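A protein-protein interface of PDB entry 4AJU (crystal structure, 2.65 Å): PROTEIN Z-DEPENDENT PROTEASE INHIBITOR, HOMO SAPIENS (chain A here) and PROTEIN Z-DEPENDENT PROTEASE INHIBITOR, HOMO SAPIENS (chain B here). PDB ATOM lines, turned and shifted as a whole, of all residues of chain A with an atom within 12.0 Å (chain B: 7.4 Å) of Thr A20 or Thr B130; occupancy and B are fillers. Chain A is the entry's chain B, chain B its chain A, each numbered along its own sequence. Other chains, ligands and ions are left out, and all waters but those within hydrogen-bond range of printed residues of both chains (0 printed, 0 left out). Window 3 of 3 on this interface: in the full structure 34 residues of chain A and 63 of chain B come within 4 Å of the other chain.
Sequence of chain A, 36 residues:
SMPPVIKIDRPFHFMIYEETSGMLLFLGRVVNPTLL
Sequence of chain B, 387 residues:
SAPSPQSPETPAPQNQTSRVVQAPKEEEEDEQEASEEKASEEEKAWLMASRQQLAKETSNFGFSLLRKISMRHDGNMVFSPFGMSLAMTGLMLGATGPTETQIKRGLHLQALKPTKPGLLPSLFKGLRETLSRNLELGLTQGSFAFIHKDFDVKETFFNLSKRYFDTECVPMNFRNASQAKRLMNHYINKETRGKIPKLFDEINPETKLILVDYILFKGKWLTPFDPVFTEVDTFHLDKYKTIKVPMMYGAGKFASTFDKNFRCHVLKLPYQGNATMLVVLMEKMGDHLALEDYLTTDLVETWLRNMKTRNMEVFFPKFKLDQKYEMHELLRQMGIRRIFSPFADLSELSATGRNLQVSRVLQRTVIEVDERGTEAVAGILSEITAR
Of the 18 printed residues of chain B, 7 touch a printed residue of chain A.
Printed residues of chain B that touch a printed residue of chain A: Ala B55, Leu B127, Thr B130, Leu B131, Leu B137, Asn B274 and Ala B275.
Printed residues of chain A that touch a printed residue of chain B: Tyr A17, Glu A18, Glu A19, Thr A20, Ser A21, Gly A22 and Met A23.
Along chain A the printed residues that touch a printed residue of chain B span positions 17 to 23.
OG1 of Thr B130 lies within hydrogen-bond range of O of Gly B126 (3.2 Å).
The side-chain carboxylate (OE2) of Glu A18 lies within hydrogen-bond range of the side-chain hydroxyl (OG1) of Thr A20 (3.0 Å).
The side-chain carboxylate (OE1) of Glu A18 lies within hydrogen-bond range of the side-chain hydroxyl (OG) of Ser A21 (2.5 Å).
The backbone carbonyl oxygen of Met A23 sits at hydrogen-bond distance from the backbone NH of Glu A18 (3.0 Å).
The side-chain hydroxyl of Ser A21 lies within hydrogen-bond range of the backbone NH of Met A23, 3.3 Å away.
Among the printed residues, pairs that only touch across the chains: Ser A21 with Ala B55, Tyr A17 with Ala B275, Ser A21 with Thr B130, Gly A22 with Ala B55, Glu A18 with Asn B274, Glu A18 with Leu B137, Glu A18 with Leu B131, Thr A20 with Thr B130, Ser A21 with Leu B131, Met A23 with Leu B127 and Met A23 with Ala B55.
N of Glu A19 is in hydrogen-bond range of O of Asn B274, 3.0 Å away.
The side-chain amide oxygen of Asn B274 is in hydrogen-bond range of the side-chain hydroxyl of Thr A20, at 2.8 Å.
O of Ala B275 lies close to OE2 of Glu A19 (3.2 Å).
Of chain B, only Thr B130 and Asn B274 come within 4 Å of Thr A20.
Printed residues of chain A within 4 Å of Thr B130: Thr A20 (3.8 Å) and Ser A21 (3.4 Å).
No residue of chain A comes within 4 Å of Gly B126.
Leu B131 touches two residues of chain A.
Of chain A, only Glu A18, Glu A19 and Thr A20 come within 4 Å of Asn B274.
Printed residues of chain B within 4 Å of Met A23: Ala B55 and Leu B127.
Of the printed residues of chain A, Ala B275 touches Tyr A17 (3.3 Å) and Glu A19 (3.2 Å).
Of the printed residues of chain B, Glu A19 touches Asn B274 and Ala B275.
Arg B128 touches none of the printed residues of chain A.
Leu A25 touches none of the printed residues of chain B.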
ATOM      1  N   ILE A  16      -5.124  -0.994  22.500  1.00  0.00           N
ATOM      2  CA  ILE A  16      -6.330  -1.560  21.886  1.00  0.00           C
ATOM      3  C   ILE A  16      -6.579  -0.905  20.538  1.00  0.00           C
ATOM      4  O   ILE A  16      -6.823   0.300  20.463  1.00  0.00           O
ATOM      5  CB  ILE A  16      -7.561  -1.384  22.749  1.00  0.00           C
ATOM      6  CG1 ILE A  16      -7.393  -2.133  24.080  1.00  0.00           C
ATOM      7  CG2 ILE A  16      -8.782  -1.897  22.008  1.00  0.00           C
ATOM      8  CD1 ILE A  16      -8.514  -1.884  25.073  1.00  0.00           C
ATOM      9  N   TYR A  17      -6.512  -1.710  19.482  1.00  0.00           N
ATOM     10  CA  TYR A  17      -6.620  -1.241  18.108  1.00  0.00           C
ATOM     11  C   TYR A  17      -7.884  -1.773  17.468  1.00  0.00           C
ATOM     12  O   TYR A  17      -8.257  -2.920  17.723  1.00  0.00           O
ATOM     13  CB  TYR A  17      -5.466  -1.788  17.282  1.00  0.00           C
ATOM     14  CG  TYR A  17      -4.249  -0.917  17.207  1.00  0.00           C
ATOM     15  CD1 TYR A  17      -4.223   0.197  16.376  1.00  0.00           C
ATOM     16  CD2 TYR A  17      -3.102  -1.233  17.926  1.00  0.00           C
ATOM     17  CE1 TYR A  17      -3.097   0.993  16.282  1.00  0.00           C
ATOM     18  CE2 TYR A  17      -1.972  -0.445  17.845  1.00  0.00           C
ATOM     19  CZ  TYR A  17      -1.970   0.669  17.022  1.00  0.00           C
ATOM     20  OH  TYR A  17      -0.837   1.455  16.923  1.00  0.00           O
ATOM     21  N   GLU A  18      -8.527  -0.956  16.631  1.00  0.00           N
ATOM     22  CA  GLU A  18      -9.558  -1.450  15.730  1.00  0.00           C
ATOM     23  C   GLU A  18      -8.872  -1.753  14.415  1.00  0.00           C
ATOM     24  O   GLU A  18      -8.379  -0.849  13.752  1.00  0.00           O
ATOM     25  CB  GLU A  18     -10.665  -0.423  15.544  1.00  0.00           C
ATOM     26  CG  GLU A  18     -11.938  -1.005  14.931  1.00  0.00           C
ATOM     27  CD  GLU A  18     -11.825  -1.232  13.433  1.00  0.00           C
ATOM     28  OE1 GLU A  18     -11.450  -0.269  12.716  1.00  0.00           O
ATOM     29  OE2 GLU A  18     -12.107  -2.371  12.973  1.00  0.00           O
ATOM     30  N   GLU A  19      -8.854  -3.026  14.037  1.00  0.00           N
ATOM     31  CA  GLU A  19      -7.915  -3.509  13.020  1.00  0.00           C
ATOM     32  C   GLU A  19      -8.276  -3.128  11.593  1.00  0.00           C
ATOM     33  O   GLU A  19      -7.400  -3.066  10.738  1.00  0.00           O
ATOM     34  CB  GLU A  19      -7.735  -5.022  13.137  1.00  0.00           C
ATOM     35  CG  GLU A  19      -7.253  -5.473  14.532  1.00  0.00           C
ATOM     36  CD  GLU A  19      -6.960  -6.961  14.600  1.00  0.00           C
ATOM     37  OE1 GLU A  19      -5.919  -7.378  14.048  1.00  0.00           O
ATOM     38  OE2 GLU A  19      -7.763  -7.710  15.208  1.00  0.00           O
ATOM     39  N   THR A  20      -9.549  -2.856  11.333  1.00  0.00           N
ATOM     40  CA  THR A  20      -9.980  -2.475   9.993  1.00  0.00           C
ATOM     41  C   THR A  20      -9.492  -1.068   9.641  1.00  0.00           C
ATOM     42  O   THR A  20      -8.848  -0.878   8.612  1.00  0.00           O
ATOM     43  CB  THR A  20     -11.519  -2.559   9.846  1.00  0.00           C
ATOM     44  OG1 THR A  20     -11.989  -3.802  10.391  1.00  0.00           O
ATOM     45  CG2 THR A  20     -11.932  -2.449   8.376  1.00  0.00           C
ATOM     46  N   SER A  21      -9.800  -0.095  10.501  1.00  0.00           N
ATOM     47  CA  SER A  21      -9.372   1.297  10.316  1.00  0.00           C
ATOM     48  C   SER A  21      -7.921   1.514  10.727  1.00  0.00           C
ATOM     49  O   SER A  21      -7.231   2.350  10.155  1.00  0.00           O
ATOM     50  CB  SER A  21     -10.244   2.239  11.142  1.00  0.00           C
ATOM     51  OG  SER A  21     -10.182   1.894  12.517  1.00  0.00           O
ATOM     52  N   GLY A  22      -7.470   0.775  11.732  1.00  0.00           N
ATOM     53  CA  GLY A  22      -6.127   0.944  12.276  1.00  0.00           C
ATOM     54  C   GLY A  22      -6.077   1.989  13.378  1.00  0.00           C
ATOM     55  O   GLY A  22      -4.996   2.480  13.730  1.00  0.00           O
ATOM     56  N   MET A  23      -7.235   2.327  13.942  1.00  0.00           N
ATOM     57  CA  MET A  23      -7.290   3.368  14.960  1.00  0.00           C
ATOM     58  C   MET A  23      -6.872   2.825  16.315  1.00  0.00           C
ATOM     59  O   MET A  23      -7.331   1.779  16.744  1.00  0.00           O
ATOM     60  CB  MET A  23      -8.690   3.982  15.054  1.00  0.00           C
ATOM     61  CG  MET A  23      -9.009   4.934  13.937  1.00  0.00           C
ATOM     62  SD  MET A  23      -7.999   6.419  14.026  1.00  0.00           S
ATOM     63  CE  MET A  23      -8.572   7.347  12.601  1.00  0.00           C
ATOM     64  N   LEU A  24      -5.985   3.564  16.971  1.00  0.00           N
ATOM     65  CA  LEU A  24      -5.565   3.284  18.332  1.00  0.00           C
ATOM     66  C   LEU A  24      -6.630   3.828  19.279  1.00  0.00           C
ATOM     67  O   LEU A  24      -6.685   5.021  19.520  1.00  0.00           O
ATOM     68  CB  LEU A  24      -4.210   3.949  18.608  1.00  0.00           C
ATOM     69  CG  LEU A  24      -3.536   3.633  19.944  1.00  0.00           C
ATOM     70  CD1 LEU A  24      -3.365   2.123  20.122  1.00  0.00           C
ATOM     71  CD2 LEU A  24      -2.201   4.352  20.041  1.00  0.00           C
ATOM     72  N   LEU A  25      -7.478   2.942  19.796  1.00  0.00           N
ATOM     73  CA  LEU A  25      -8.577   3.341  20.656  1.00  0.00           C
ATOM     74  C   LEU A  25      -8.124   3.655  22.069  1.00  0.00           C
ATOM     75  O   LEU A  25      -8.587   4.631  22.669  1.00  0.00           O
ATOM     76  CB  LEU A  25      -9.613   2.235  20.743  1.00  0.00           C
ATOM     77  CG  LEU A  25     -10.292   1.824  19.451  1.00  0.00           C
ATOM     78  CD1 LEU A  25     -11.351   0.787  19.790  1.00  0.00           C
ATOM     79  CD2 LEU A  25     -10.884   3.026  18.737  1.00  0.00           C
ATOM     80  N   ARG B  51      -7.319   7.732   4.784  1.00  0.00           N
ATOM     81  CA  ARG B  51      -7.752   7.069   6.018  1.00  0.00           C
ATOM     82  C   ARG B  51      -6.615   6.297   6.682  1.00  0.00           C
ATOM     83  O   ARG B  51      -6.504   6.291   7.904  1.00  0.00           O
ATOM     84  CB  ARG B  51      -8.956   6.157   5.767  1.00  0.00           C
ATOM     85  CG  ARG B  51     -10.308   6.801   6.131  1.00  0.00           C
ATOM     86  CD  ARG B  51     -11.487   6.138   5.410  1.00  0.00           C
ATOM     87  NE  ARG B  51     -11.210   4.735   5.085  1.00  0.00           N
ATOM     88  CZ  ARG B  51     -11.884   4.014   4.192  1.00  0.00           C
ATOM     89  NH1 ARG B  51     -12.917   4.535   3.530  1.00  0.00           N
ATOM     90  NH2 ARG B  51     -11.521   2.752   3.965  1.00  0.00           N
ATOM     91  N   GLN B  52      -5.773   5.654   5.883  1.00  0.00           N
ATOM     92  CA  GLN B  52      -4.561   5.041   6.409  1.00  0.00           C
ATOM     93  C   GLN B  52      -3.656   6.099   7.030  1.00  0.00           C
ATOM     94  O   GLN B  52      -3.088   5.877   8.098  1.00  0.00           O
ATOM     95  CB  GLN B  52      -3.806   4.274   5.318  1.00  0.00           C
ATOM     96  CG  GLN B  52      -4.503   2.993   4.880  1.00  0.00           C
ATOM     97  CD  GLN B  52      -3.731   2.229   3.817  1.00  0.00           C
ATOM     98  OE1 GLN B  52      -2.544   1.933   3.982  1.00  0.00           O
ATOM     99  NE2 GLN B  52      -4.407   1.894   2.721  1.00  0.00           N
ATOM    100  N   ALA B  55      -5.107   7.159  10.459  1.00  0.00           N
ATOM    101  CA  ALA B  55      -4.918   6.141  11.495  1.00  0.00           C
ATOM    102  C   ALA B  55      -3.488   6.181  12.017  1.00  0.00           C
ATOM    103  O   ALA B  55      -3.253   6.149  13.224  1.00  0.00           O
ATOM    104  CB  ALA B  55      -5.231   4.767  10.949  1.00  0.00           C
ATOM    105  N   PHE B 124     -14.762  11.788   7.015  1.00  0.00           N
ATOM    106  CA  PHE B 124     -15.446  11.427   8.258  1.00  0.00           C
ATOM    107  C   PHE B 124     -16.537  10.391   8.039  1.00  0.00           C
ATOM    108  O   PHE B 124     -16.761   9.531   8.886  1.00  0.00           O
ATOM    109  CB  PHE B 124     -16.052  12.667   8.925  1.00  0.00           C
ATOM    110  CG  PHE B 124     -15.100  13.397   9.824  1.00  0.00           C
ATOM    111  CD1 PHE B 124     -14.713  12.841  11.038  1.00  0.00           C
ATOM    112  CD2 PHE B 124     -14.594  14.637   9.464  1.00  0.00           C
ATOM    113  CE1 PHE B 124     -13.836  13.505  11.877  1.00  0.00           C
ATOM    114  CE2 PHE B 124     -13.717  15.314  10.300  1.00  0.00           C
ATOM    115  CZ  PHE B 124     -13.338  14.748  11.509  1.00  0.00           C
ATOM    116  N   LYS B 125     -17.232  10.492   6.910  1.00  0.00           N
ATOM    117  CA  LYS B 125     -18.243   9.510   6.537  1.00  0.00           C
ATOM    118  C   LYS B 125     -17.597   8.138   6.399  1.00  0.00           C
ATOM    119  O   LYS B 125     -18.147   7.140   6.857  1.00  0.00           O
ATOM    120  CB  LYS B 125     -18.926   9.912   5.228  1.00  0.00           C
ATOM    121  CG  LYS B 125     -20.109   9.028   4.845  1.00  0.00           C
ATOM    122  CD  LYS B 125     -20.749   9.466   3.528  1.00  0.00           C
ATOM    123  CE  LYS B 125     -21.539   8.339   2.871  1.00  0.00           C
ATOM    124  NZ  LYS B 125     -22.128   8.763   1.573  1.00  0.00           N
ATOM    125  N   GLY B 126     -16.422   8.106   5.777  1.00  0.00           N
ATOM    126  CA  GLY B 126     -15.666   6.876   5.588  1.00  0.00           C
ATOM    127  C   GLY B 126     -15.181   6.255   6.883  1.00  0.00           C
ATOM    128  O   GLY B 126     -15.091   5.028   6.997  1.00  0.00           O
ATOM    129  N   LEU B 127     -14.863   7.098   7.860  1.00  0.00           N
ATOM    130  CA  LEU B 127     -14.406   6.612   9.150  1.00  0.00           C
ATOM    131  C   LEU B 127     -15.553   5.964   9.928  1.00  0.00           C
ATOM    132  O   LEU B 127     -15.385   4.879  10.481  1.00  0.00           O
ATOM    133  CB  LEU B 127     -13.761   7.741   9.953  1.00  0.00           C
ATOM    134  CG  LEU B 127     -12.967   7.328  11.198  1.00  0.00           C
ATOM    135  CD1 LEU B 127     -11.954   6.237  10.882  1.00  0.00           C
ATOM    136  CD2 LEU B 127     -12.273   8.541  11.774  1.00  0.00           C
ATOM    137  N   ARG B 128     -16.711   6.622   9.961  1.00  0.00           N
ATOM    138  CA  ARG B 128     -17.916   6.044  10.574  1.00  0.00           C
ATOM    139  C   ARG B 128     -18.278   4.703   9.978  1.00  0.00           C
ATOM    140  O   ARG B 128     -18.616   3.784  10.709  1.00  0.00           O
ATOM    141  CB  ARG B 128     -19.126   6.960  10.403  1.00  0.00           C
ATOM    142  CG  ARG B 128     -19.093   8.181  11.269  1.00  0.00           C
ATOM    143  CD  ARG B 128     -20.475   8.779  11.467  1.00  0.00           C
ATOM    144  NE  ARG B 128     -20.468   9.647  12.643  1.00  0.00           N
ATOM    145  CZ  ARG B 128     -20.478   9.220  13.910  1.00  0.00           C
ATOM    146  NH1 ARG B 128     -20.517   7.919  14.210  1.00  0.00           N
ATOM    147  NH2 ARG B 128     -20.458  10.110  14.896  1.00  0.00           N
ATOM    148  N   GLU B 129     -18.229   4.605   8.653  1.00  0.00           N
ATOM    149  CA  GLU B 129     -18.539   3.357   7.958  1.00  0.00           C
ATOM    150  C   GLU B 129     -17.646   2.233   8.455  1.00  0.00           C
ATOM    151  O   GLU B 129     -18.131   1.166   8.822  1.00  0.00           O
ATOM    152  CB  GLU B 129     -18.363   3.520   6.447  1.00  0.00           C
ATOM    153  CG  GLU B 129     -18.466   2.221   5.655  1.00  0.00           C
ATOM    154  CD  GLU B 129     -18.381   2.437   4.157  1.00  0.00           C
ATOM    155  OE1 GLU B 129     -17.700   3.379   3.713  1.00  0.00           O
ATOM    156  OE2 GLU B 129     -18.996   1.653   3.413  1.00  0.00           O
ATOM    157  N   THR B 130     -16.340   2.488   8.464  1.00  0.00           N
ATOM    158  CA  THR B 130     -15.350   1.505   8.872  1.00  0.00           C
ATOM    159  C   THR B 130     -15.565   1.074  10.318  1.00  0.00           C
ATOM    160  O   THR B 130     -15.466  -0.114  10.634  1.00  0.00           O
ATOM    161  CB  THR B 130     -13.925   2.065   8.673  1.00  0.00           C
ATOM    162  OG1 THR B 130     -13.668   2.203   7.268  1.00  0.00           O
ATOM    163  CG2 THR B 130     -12.886   1.152   9.263  1.00  0.00           C
ATOM    164  N   LEU B 131     -15.879   2.032  11.187  1.00  0.00           N
ATOM    165  CA  LEU B 131     -16.168   1.741  12.591  1.00  0.00           C
ATOM    166  C   LEU B 131     -17.590   1.203  12.831  1.00  0.00           C
ATOM    167  O   LEU B 131     -17.941   0.873  13.960  1.00  0.00           O
ATOM    168  CB  LEU B 131     -15.947   2.994  13.439  1.00  0.00           C
ATOM    169  CG  LEU B 131     -14.508   3.515  13.531  1.00  0.00           C
ATOM    170  CD1 LEU B 131     -14.473   4.830  14.275  1.00  0.00           C
ATOM    171  CD2 LEU B 131     -13.583   2.511  14.209  1.00  0.00           C
ATOM    172  N   SER B 132     -18.401   1.121  11.781  1.00  0.00           N
ATOM    173  CA  SER B 132     -19.769   0.606  11.882  1.00  0.00           C
ATOM    174  C   SER B 132     -19.979  -0.745  11.209  1.00  0.00           C
ATOM    175  O   SER B 132     -20.914  -1.462  11.564  1.00  0.00           O
ATOM    176  CB  SER B 132     -20.750   1.595  11.258  1.00  0.00           C
ATOM    177  OG  SER B 132     -20.776   2.799  11.991  1.00  0.00           O
ATOM    178  N   ARG B 133     -19.146  -1.076  10.225  1.00  0.00           N
ATOM    179  CA  ARG B 133     -19.347  -2.292   9.428  1.00  0.00           C
ATOM    180  C   ARG B 133     -19.408  -3.561  10.262  1.00  0.00           C
ATOM    181  O   ARG B 133     -20.229  -4.423  10.001  1.00  0.00           O
ATOM    182  CB  ARG B 133     -18.294  -2.442   8.314  1.00  0.00           C
ATOM    183  CG  ARG B 133     -16.848  -2.245   8.733  1.00  0.00           C
ATOM    184  CD  ARG B 133     -15.897  -2.505   7.564  1.00  0.00           C
ATOM    185  NE  ARG B 133     -15.763  -3.932   7.277  1.00  0.00           N
ATOM    186  CZ  ARG B 133     -15.237  -4.445   6.167  1.00  0.00           C
ATOM    187  NH1 ARG B 133     -14.783  -3.653   5.196  1.00  0.00           N
ATOM    188  NH2 ARG B 133     -15.174  -5.768   6.022  1.00  0.00           N
ATOM    189  N   ASN B 134     -18.557  -3.673  11.273  1.00  0.00           N
ATOM    190  CA  ASN B 134     -18.538  -4.874  12.093  1.00  0.00           C
ATOM    191  C   ASN B 134     -19.398  -4.727  13.338  1.00  0.00           C
ATOM    192  O   ASN B 134     -19.023  -4.054  14.291  1.00  0.00           O
ATOM    193  CB  ASN B 134     -17.110  -5.253  12.465  1.00  0.00           C
ATOM    194  CG  ASN B 134     -16.989  -6.708  12.832  1.00  0.00           C
ATOM    195  OD1 ASN B 134     -17.810  -7.246  13.583  1.00  0.00           O
ATOM    196  ND2 ASN B 134     -15.972  -7.361  12.297  1.00  0.00           N
ATOM    197  N   LEU B 137     -18.099  -5.316  17.172  1.00  0.00           N
ATOM    198  CA  LEU B 137     -16.982  -4.538  17.708  1.00  0.00           C
ATOM    199  C   LEU B 137     -17.217  -4.079  19.137  1.00  0.00           C
ATOM    200  O   LEU B 137     -16.313  -4.159  19.964  1.00  0.00           O
ATOM    201  CB  LEU B 137     -16.685  -3.319  16.832  1.00  0.00           C
ATOM    202  CG  LEU B 137     -15.529  -2.424  17.305  1.00  0.00           C
ATOM    203  CD1 LEU B 137     -14.235  -3.211  17.406  1.00  0.00           C
ATOM    204  CD2 LEU B 137     -15.363  -1.224  16.378  1.00  0.00           C
ATOM    205  N   GLY B 273     -15.180  -8.891  16.697  1.00  0.00           N
ATOM    206  CA  GLY B 273     -15.465  -7.684  15.927  1.00  0.00           C
ATOM    207  C   GLY B 273     -14.250  -7.018  15.304  1.00  0.00           C
ATOM    208  O   GLY B 273     -14.284  -5.827  14.948  1.00  0.00           O
ATOM    209  N   ASN B 274     -13.174  -7.784  15.182  1.00  0.00           N
ATOM    210  CA  ASN B 274     -11.969  -7.339  14.507  1.00  0.00           C
ATOM    211  C   ASN B 274     -11.219  -6.212  15.226  1.00  0.00           C
ATOM    212  O   ASN B 274     -10.675  -5.314  14.602  1.00  0.00           O
ATOM    213  CB  ASN B 274     -12.295  -6.948  13.074  1.00  0.00           C
ATOM    214  CG  ASN B 274     -11.095  -7.019  12.176  1.00  0.00           C
ATOM    215  OD1 ASN B 274     -10.678  -6.016  11.597  1.00  0.00           O
ATOM    216  ND2 ASN B 274     -10.512  -8.206  12.066  1.00  0.00           N
ATOM    217  N   ALA B 275     -11.207  -6.276  16.548  1.00  0.00           N
ATOM    218  CA  ALA B 275     -10.343  -5.442  17.370  1.00  0.00           C
ATOM    219  C   ALA B 275      -9.318  -6.356  18.029  1.00  0.00           C
ATOM    220  O   ALA B 275      -9.436  -7.574  17.951  1.00  0.00           O
ATOM    221  CB  ALA B 275     -11.154  -4.700  18.420  1.00  0.00           C
